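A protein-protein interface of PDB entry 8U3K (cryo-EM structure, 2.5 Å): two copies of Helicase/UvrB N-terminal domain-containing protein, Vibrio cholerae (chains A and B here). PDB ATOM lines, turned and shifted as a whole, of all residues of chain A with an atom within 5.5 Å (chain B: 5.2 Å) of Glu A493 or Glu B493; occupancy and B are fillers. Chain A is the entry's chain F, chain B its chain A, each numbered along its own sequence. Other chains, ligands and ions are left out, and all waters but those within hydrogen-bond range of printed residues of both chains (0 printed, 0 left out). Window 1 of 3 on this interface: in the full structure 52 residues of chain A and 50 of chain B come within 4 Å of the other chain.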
ATOM      1  N   TRP A 325      -7.278 -18.089  -0.335  1.00  0.00           N
ATOM      2  CA  TRP A 325      -7.619 -16.826   0.302  1.00  0.00           C
ATOM      3  C   TRP A 325      -8.441 -17.049   1.560  1.00  0.00           C
ATOM      4  O   TRP A 325      -8.222 -16.387   2.576  1.00  0.00           O
ATOM      5  CB  TRP A 325      -8.383 -15.935  -0.675  1.00  0.00           C
ATOM      6  CG  TRP A 325      -8.941 -14.719  -0.023  1.00  0.00           C
ATOM      7  CD1 TRP A 325      -8.311 -13.536   0.161  1.00  0.00           C
ATOM      8  CD2 TRP A 325     -10.234 -14.578   0.566  1.00  0.00           C
ATOM      9  NE1 TRP A 325      -9.128 -12.660   0.815  1.00  0.00           N
ATOM     10  CE2 TRP A 325     -10.317 -13.281   1.080  1.00  0.00           C
ATOM     11  CE3 TRP A 325     -11.329 -15.428   0.708  1.00  0.00           C
ATOM     12  CZ2 TRP A 325     -11.447 -12.811   1.720  1.00  0.00           C
ATOM     13  CZ3 TRP A 325     -12.440 -14.963   1.346  1.00  0.00           C
ATOM     14  CH2 TRP A 325     -12.498 -13.666   1.841  1.00  0.00           C
ATOM     15  N   THR A 329      -7.169 -15.960   5.234  1.00  0.00           N
ATOM     16  CA  THR A 329      -7.924 -14.994   6.026  1.00  0.00           C
ATOM     17  C   THR A 329      -8.356 -15.577   7.360  1.00  0.00           C
ATOM     18  O   THR A 329      -8.311 -14.887   8.380  1.00  0.00           O
ATOM     19  CB  THR A 329      -9.149 -14.511   5.259  1.00  0.00           C
ATOM     20  OG1 THR A 329      -9.786 -15.626   4.629  1.00  0.00           O
ATOM     21  CG2 THR A 329      -8.758 -13.516   4.224  1.00  0.00           C
ATOM     22  N   ASN A 490     -13.204  -9.906  13.025  1.00  0.00           N
ATOM     23  CA  ASN A 490     -12.725  -9.203  11.838  1.00  0.00           C
ATOM     24  C   ASN A 490     -12.832 -10.091  10.602  1.00  0.00           C
ATOM     25  O   ASN A 490     -11.906 -10.205   9.802  1.00  0.00           O
ATOM     26  CB  ASN A 490     -11.300  -8.694  12.041  1.00  0.00           C
ATOM     27  CG  ASN A 490     -10.911  -7.646  11.051  1.00  0.00           C
ATOM     28  OD1 ASN A 490      -9.978  -7.826  10.289  1.00  0.00           O
ATOM     29  ND2 ASN A 490     -11.625  -6.540  11.054  1.00  0.00           N
ATOM     30  N   LEU A 491     -13.990 -10.720  10.447  1.00  0.00           N
ATOM     31  CA  LEU A 491     -14.240 -11.644   9.351  1.00  0.00           C
ATOM     32  C   LEU A 491     -15.475 -11.237   8.568  1.00  0.00           C
ATOM     33  O   LEU A 491     -16.242 -12.089   8.135  1.00  0.00           O
ATOM     34  CB  LEU A 491     -14.388 -13.071   9.866  1.00  0.00           C
ATOM     35  CG  LEU A 491     -13.122 -13.737  10.390  1.00  0.00           C
ATOM     36  CD1 LEU A 491     -13.484 -14.971  11.134  1.00  0.00           C
ATOM     37  CD2 LEU A 491     -12.187 -14.077   9.267  1.00  0.00           C
ATOM     38  N   GLN A 492     -15.670  -9.935   8.367  1.00  0.00           N
ATOM     39  CA  GLN A 492     -16.866  -9.457   7.684  1.00  0.00           C
ATOM     40  C   GLN A 492     -16.887  -9.868   6.222  1.00  0.00           C
ATOM     41  O   GLN A 492     -17.937  -9.807   5.578  1.00  0.00           O
ATOM     42  CB  GLN A 492     -16.963  -7.939   7.792  1.00  0.00           C
ATOM     43  CG  GLN A 492     -17.102  -7.412   9.195  1.00  0.00           C
ATOM     44  CD  GLN A 492     -15.775  -7.046   9.802  1.00  0.00           C
ATOM     45  OE1 GLN A 492     -14.782  -7.729   9.593  1.00  0.00           O
ATOM     46  NE2 GLN A 492     -15.746  -5.958  10.547  1.00  0.00           N
ATOM     47  N   GLU A 493     -15.743 -10.276   5.677  1.00  0.00           N
ATOM     48  CA  GLU A 493     -15.682 -10.700   4.287  1.00  0.00           C
ATOM     49  C   GLU A 493     -16.437 -11.995   4.042  1.00  0.00           C
ATOM     50  O   GLU A 493     -16.762 -12.301   2.893  1.00  0.00           O
ATOM     51  CB  GLU A 493     -14.225 -10.857   3.872  1.00  0.00           C
ATOM     52  CG  GLU A 493     -13.311  -9.859   4.551  1.00  0.00           C
ATOM     53  CD  GLU A 493     -12.049  -9.579   3.762  1.00  0.00           C
ATOM     54  OE1 GLU A 493     -10.947  -9.840   4.285  1.00  0.00           O
ATOM     55  OE2 GLU A 493     -12.159  -9.101   2.618  1.00  0.00           O
ATOM     56  N   PHE A 494     -16.724 -12.758   5.087  1.00  0.00           N
ATOM     57  CA  PHE A 494     -17.408 -14.033   4.963  1.00  0.00           C
ATOM     58  C   PHE A 494     -18.904 -13.925   5.171  1.00  0.00           C
ATOM     59  O   PHE A 494     -19.558 -14.953   5.339  1.00  0.00           O
ATOM     60  CB  PHE A 494     -16.846 -15.034   5.965  1.00  0.00           C
ATOM     61  CG  PHE A 494     -15.512 -15.566   5.591  1.00  0.00           C
ATOM     62  CD1 PHE A 494     -15.393 -16.561   4.654  1.00  0.00           C
ATOM     63  CD2 PHE A 494     -14.376 -15.077   6.181  1.00  0.00           C
ATOM     64  CE1 PHE A 494     -14.166 -17.050   4.313  1.00  0.00           C
ATOM     65  CE2 PHE A 494     -13.152 -15.566   5.841  1.00  0.00           C
ATOM     66  CZ  PHE A 494     -13.046 -16.552   4.908  1.00  0.00           C
ATOM     67  N   GLU A 495     -19.450 -12.712   5.175  1.00  0.00           N
ATOM     68  CA  GLU A 495     -20.851 -12.517   5.523  1.00  0.00           C
ATOM     69  C   GLU A 495     -21.772 -13.214   4.535  1.00  0.00           C
ATOM     70  O   GLU A 495     -22.675 -13.963   4.928  1.00  0.00           O
ATOM     71  CB  GLU A 495     -21.153 -11.024   5.576  1.00  0.00           C
ATOM     72  CG  GLU A 495     -22.526 -10.690   6.082  1.00  0.00           C
ATOM     73  CD  GLU A 495     -22.687  -9.221   6.382  1.00  0.00           C
ATOM     74  OE1 GLU A 495     -21.696  -8.587   6.798  1.00  0.00           O
ATOM     75  OE2 GLU A 495     -23.806  -8.697   6.206  1.00  0.00           O
ATOM     76  N   SER A 496     -21.547 -12.988   3.243  1.00  0.00           N
ATOM     77  CA  SER A 496     -22.395 -13.594   2.228  1.00  0.00           C
ATOM     78  C   SER A 496     -22.268 -15.107   2.237  1.00  0.00           C
ATOM     79  O   SER A 496     -23.254 -15.818   2.025  1.00  0.00           O
ATOM     80  CB  SER A 496     -22.040 -13.035   0.857  1.00  0.00           C
ATOM     81  OG  SER A 496     -20.670 -13.236   0.582  1.00  0.00           O
ATOM     82  N   ALA A 497     -21.065 -15.619   2.483  1.00  0.00           N
ATOM     83  CA  ALA A 497     -20.874 -17.061   2.549  1.00  0.00           C
ATOM     84  C   ALA A 497     -21.666 -17.672   3.693  1.00  0.00           C
ATOM     85  O   ALA A 497     -22.305 -18.717   3.527  1.00  0.00           O
ATOM     86  CB  ALA A 497     -19.392 -17.380   2.691  1.00  0.00           C
ATOM     87  N   TRP B 325     -11.629  -1.739  10.972  1.00  0.00           N
ATOM     88  CA  TRP B 325     -11.501  -2.923  10.137  1.00  0.00           C
ATOM     89  C   TRP B 325     -10.240  -2.866   9.295  1.00  0.00           C
ATOM     90  O   TRP B 325      -9.556  -3.878   9.129  1.00  0.00           O
ATOM     91  CB  TRP B 325     -12.728  -3.071   9.239  1.00  0.00           C
ATOM     92  CG  TRP B 325     -12.547  -4.108   8.183  1.00  0.00           C
ATOM     93  CD1 TRP B 325     -12.807  -5.432   8.292  1.00  0.00           C
ATOM     94  CD2 TRP B 325     -12.048  -3.908   6.859  1.00  0.00           C
ATOM     95  NE1 TRP B 325     -12.504  -6.073   7.125  1.00  0.00           N
ATOM     96  CE2 TRP B 325     -12.032  -5.155   6.228  1.00  0.00           C
ATOM     97  CE3 TRP B 325     -11.606  -2.793   6.151  1.00  0.00           C
ATOM     98  CZ2 TRP B 325     -11.599  -5.321   4.925  1.00  0.00           C
ATOM     99  CZ3 TRP B 325     -11.175  -2.959   4.863  1.00  0.00           C
ATOM    100  CH2 TRP B 325     -11.176  -4.208   4.260  1.00  0.00           C
ATOM    101  N   THR B 329      -7.271  -5.595   9.587  1.00  0.00           N
ATOM    102  CA  THR B 329      -6.895  -6.423   8.446  1.00  0.00           C
ATOM    103  C   THR B 329      -5.435  -6.237   8.075  1.00  0.00           C
ATOM    104  O   THR B 329      -4.749  -7.207   7.747  1.00  0.00           O
ATOM    105  CB  THR B 329      -7.766  -6.106   7.239  1.00  0.00           C
ATOM    106  OG1 THR B 329      -7.904  -4.690   7.112  1.00  0.00           O
ATOM    107  CG2 THR B 329      -9.116  -6.714   7.392  1.00  0.00           C
ATOM    108  N   ASN B 333      -2.746  -9.366   8.387  1.00  0.00           N
ATOM    109  CA  ASN B 333      -2.192  -9.948   7.173  1.00  0.00           C
ATOM    110  C   ASN B 333      -0.721  -9.612   6.994  1.00  0.00           C
ATOM    111  O   ASN B 333       0.003 -10.354   6.330  1.00  0.00           O
ATOM    112  CB  ASN B 333      -2.997  -9.489   5.968  1.00  0.00           C
ATOM    113  CG  ASN B 333      -4.330 -10.162   5.884  1.00  0.00           C
ATOM    114  OD1 ASN B 333      -4.419 -11.333   5.547  1.00  0.00           O
ATOM    115  ND2 ASN B 333      -5.378  -9.437   6.209  1.00  0.00           N
ATOM    116  N   ASN B 490      -2.284 -11.184   0.794  1.00  0.00           N
ATOM    117  CA  ASN B 490      -3.649 -11.579   1.129  1.00  0.00           C
ATOM    118  C   ASN B 490      -4.495 -10.357   1.480  1.00  0.00           C
ATOM    119  O   ASN B 490      -5.291 -10.366   2.416  1.00  0.00           O
ATOM    120  CB  ASN B 490      -3.653 -12.614   2.254  1.00  0.00           C
ATOM    121  CG  ASN B 490      -4.960 -13.326   2.388  1.00  0.00           C
ATOM    122  OD1 ASN B 490      -5.610 -13.245   3.417  1.00  0.00           O
ATOM    123  ND2 ASN B 490      -5.362 -14.024   1.344  1.00  0.00           N
ATOM    124  N   LEU B 491      -4.318  -9.293   0.709  1.00  0.00           N
ATOM    125  CA  LEU B 491      -5.027  -8.042   0.936  1.00  0.00           C
ATOM    126  C   LEU B 491      -5.877  -7.667  -0.264  1.00  0.00           C
ATOM    127  O   LEU B 491      -5.886  -6.514  -0.682  1.00  0.00           O
ATOM    128  CB  LEU B 491      -4.052  -6.918   1.263  1.00  0.00           C
ATOM    129  CG  LEU B 491      -3.382  -7.010   2.624  1.00  0.00           C
ATOM    130  CD1 LEU B 491      -2.301  -5.996   2.734  1.00  0.00           C
ATOM    131  CD2 LEU B 491      -4.399  -6.796   3.700  1.00  0.00           C
ATOM    132  N   GLN B 492      -6.597  -8.634  -0.828  1.00  0.00           N
ATOM    133  CA  GLN B 492      -7.377  -8.378  -2.032  1.00  0.00           C
ATOM    134  C   GLN B 492      -8.560  -7.466  -1.760  1.00  0.00           C
ATOM    135  O   GLN B 492      -9.130  -6.900  -2.696  1.00  0.00           O
ATOM    136  CB  GLN B 492      -7.865  -9.692  -2.631  1.00  0.00           C
ATOM    137  CG  GLN B 492      -6.778 -10.559  -3.209  1.00  0.00           C
ATOM    138  CD  GLN B 492      -6.309 -11.604  -2.238  1.00  0.00           C
ATOM    139  OE1 GLN B 492      -6.263 -11.368  -1.038  1.00  0.00           O
ATOM    140  NE2 GLN B 492      -5.960 -12.772  -2.748  1.00  0.00           N
ATOM    141  N   GLU B 493      -8.953  -7.318  -0.499  1.00  0.00           N
ATOM    142  CA  GLU B 493     -10.076  -6.455  -0.163  1.00  0.00           C
ATOM    143  C   GLU B 493      -9.742  -4.981  -0.316  1.00  0.00           C
ATOM    144  O   GLU B 493     -10.654  -4.153  -0.359  1.00  0.00           O
ATOM    145  CB  GLU B 493     -10.525  -6.734   1.260  1.00  0.00           C
ATOM    146  CG  GLU B 493      -9.388  -6.719   2.248  1.00  0.00           C
ATOM    147  CD  GLU B 493      -8.849  -8.105   2.543  1.00  0.00           C
ATOM    148  OE1 GLU B 493      -8.702  -8.901   1.592  1.00  0.00           O
ATOM    149  OE2 GLU B 493      -8.557  -8.391   3.723  1.00  0.00           O
ATOM    150  N   PHE B 494      -8.467  -4.633  -0.394  1.00  0.00           N
ATOM    151  CA  PHE B 494      -8.055  -3.254  -0.581  1.00  0.00           C
ATOM    152  C   PHE B 494      -7.861  -2.894  -2.040  1.00  0.00           C
ATOM    153  O   PHE B 494      -7.259  -1.860  -2.327  1.00  0.00           O
ATOM    154  CB  PHE B 494      -6.762  -2.984   0.176  1.00  0.00           C
ATOM    155  CG  PHE B 494      -6.931  -2.935   1.650  1.00  0.00           C
ATOM    156  CD1 PHE B 494      -7.505  -1.842   2.256  1.00  0.00           C
ATOM    157  CD2 PHE B 494      -6.502  -3.974   2.435  1.00  0.00           C
ATOM    158  CE1 PHE B 494      -7.654  -1.798   3.610  1.00  0.00           C
ATOM    159  CE2 PHE B 494      -6.649  -3.929   3.789  1.00  0.00           C
ATOM    160  CZ  PHE B 494      -7.223  -2.843   4.376  1.00  0.00           C
ATOM    161  N   GLU B 495      -8.339  -3.728  -2.958  1.00  0.00           N
ATOM    162  CA  GLU B 495      -8.142  -3.479  -4.381  1.00  0.00           C
ATOM    163  C   GLU B 495      -8.815  -2.187  -4.815  1.00  0.00           C
ATOM    164  O   GLU B 495      -8.200  -1.337  -5.471  1.00  0.00           O
ATOM    165  CB  GLU B 495      -8.680  -4.664  -5.173  1.00  0.00           C
ATOM    166  CG  GLU B 495      -8.161  -4.777  -6.574  1.00  0.00           C
ATOM    167  CD  GLU B 495      -9.228  -5.251  -7.529  1.00  0.00           C
ATOM    168  OE1 GLU B 495      -8.884  -5.894  -8.541  1.00  0.00           O
ATOM    169  OE2 GLU B 495     -10.419  -4.986  -7.266  1.00  0.00           O
ATOM    170  N   SER B 496     -10.080  -2.017  -4.437  1.00  0.00           N
ATOM    171  CA  SER B 496     -10.825  -0.831  -4.835  1.00  0.00           C
ATOM    172  C   SER B 496     -10.222   0.428  -4.237  1.00  0.00           C
ATOM    173  O   SER B 496     -10.170   1.468  -4.897  1.00  0.00           O
ATOM    174  CB  SER B 496     -12.284  -0.974  -4.423  1.00  0.00           C
ATOM    175  OG  SER B 496     -12.391  -1.133  -3.023  1.00  0.00           O
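CD1 of Trp A325 touches ND2 of Asn B490, 3.2 Å away.
OE1 of Gln B492 touches CD1 of Trp A325, 3.2 Å away.
Trp A325 touches Glu B493.
Asn B490 touches Thr A329.
Asn A490 touches Trp B325 (ND2 to CD1, 3.2 Å).
OD1 of Asn A490 touches CG2 of Thr B329, at 3.2 Å.
OE1 of Gln A492 touches CD1 of Trp B325, 3.3 Å away.
Of the 10 printed residues of chain B, 5 touch a printed residue of chain A.
Along chain B the printed residues that touch a printed residue of chain A span positions 325 to 493.
Printed residues of chain A that touch a printed residue of chain B: Trp A325, Thr A329, Asn A490, Gln A492 and Glu A493.
Hydrophobic or aromatic side chains of chain A within 4 Å of the printed part of chain B: Trp A325.
Among the printed residues, 8 pairs touch across the chains.
Trp A325 touches Gln B492, and with the chains exchanged Gln A492 touches Trp B325.
Trp A325 touches Glu B493, but with the chains exchanged Glu A493 does not touch Trp B325 (4.4 Å).
Thr A329 touches Asn B490, and with the chains exchanged Asn A490 touches Thr B329.
Glu B493 touches its own counterpart, Glu A493.
Positions printed for both chains: 325, 329, 490, 491, 492, 493, 494, 495 and 496.
The side-chain hydroxyl (OG1) of Thr B329 lies within hydrogen-bond range of the backbone carbonyl oxygen (O) of Trp B325 (2.7 Å).
O of Thr B329 lies within hydrogen-bond range of ND2 of Asn B333.
OD1 of Asn B333 sits close to OD1 of Asn B490, 3.1 Å away.
The backbone carbonyl oxygen of Trp A325 is in hydrogen-bond range of the side-chain hydroxyl of Thr A329 (2.7 Å).
The side-chain carboxylate of Glu A493 lies close to the side-chain carboxylate of Glu B493 (2.9 Å).
Printed residues of chain B within 4 Å of Trp A325: Asn B490 (3.2 Å), Gln B492 (3.2 Å) and Glu B493 (3.9 Å).
Of the printed residues of chain A, Asn B490 touches Trp A325 (3.2 Å) and Thr A329 (3.3 Å).
Of the printed residues of chain A, Gln B492 touches Trp A325.
Glu B493 touches two residues of chain A.
The nearest residue of chain B that does not touch Glu A493 is Trp B325 (4.4 Å).
The nearest residue of chain A that does not touch Glu B493 is Thr A329 (5.2 Å).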
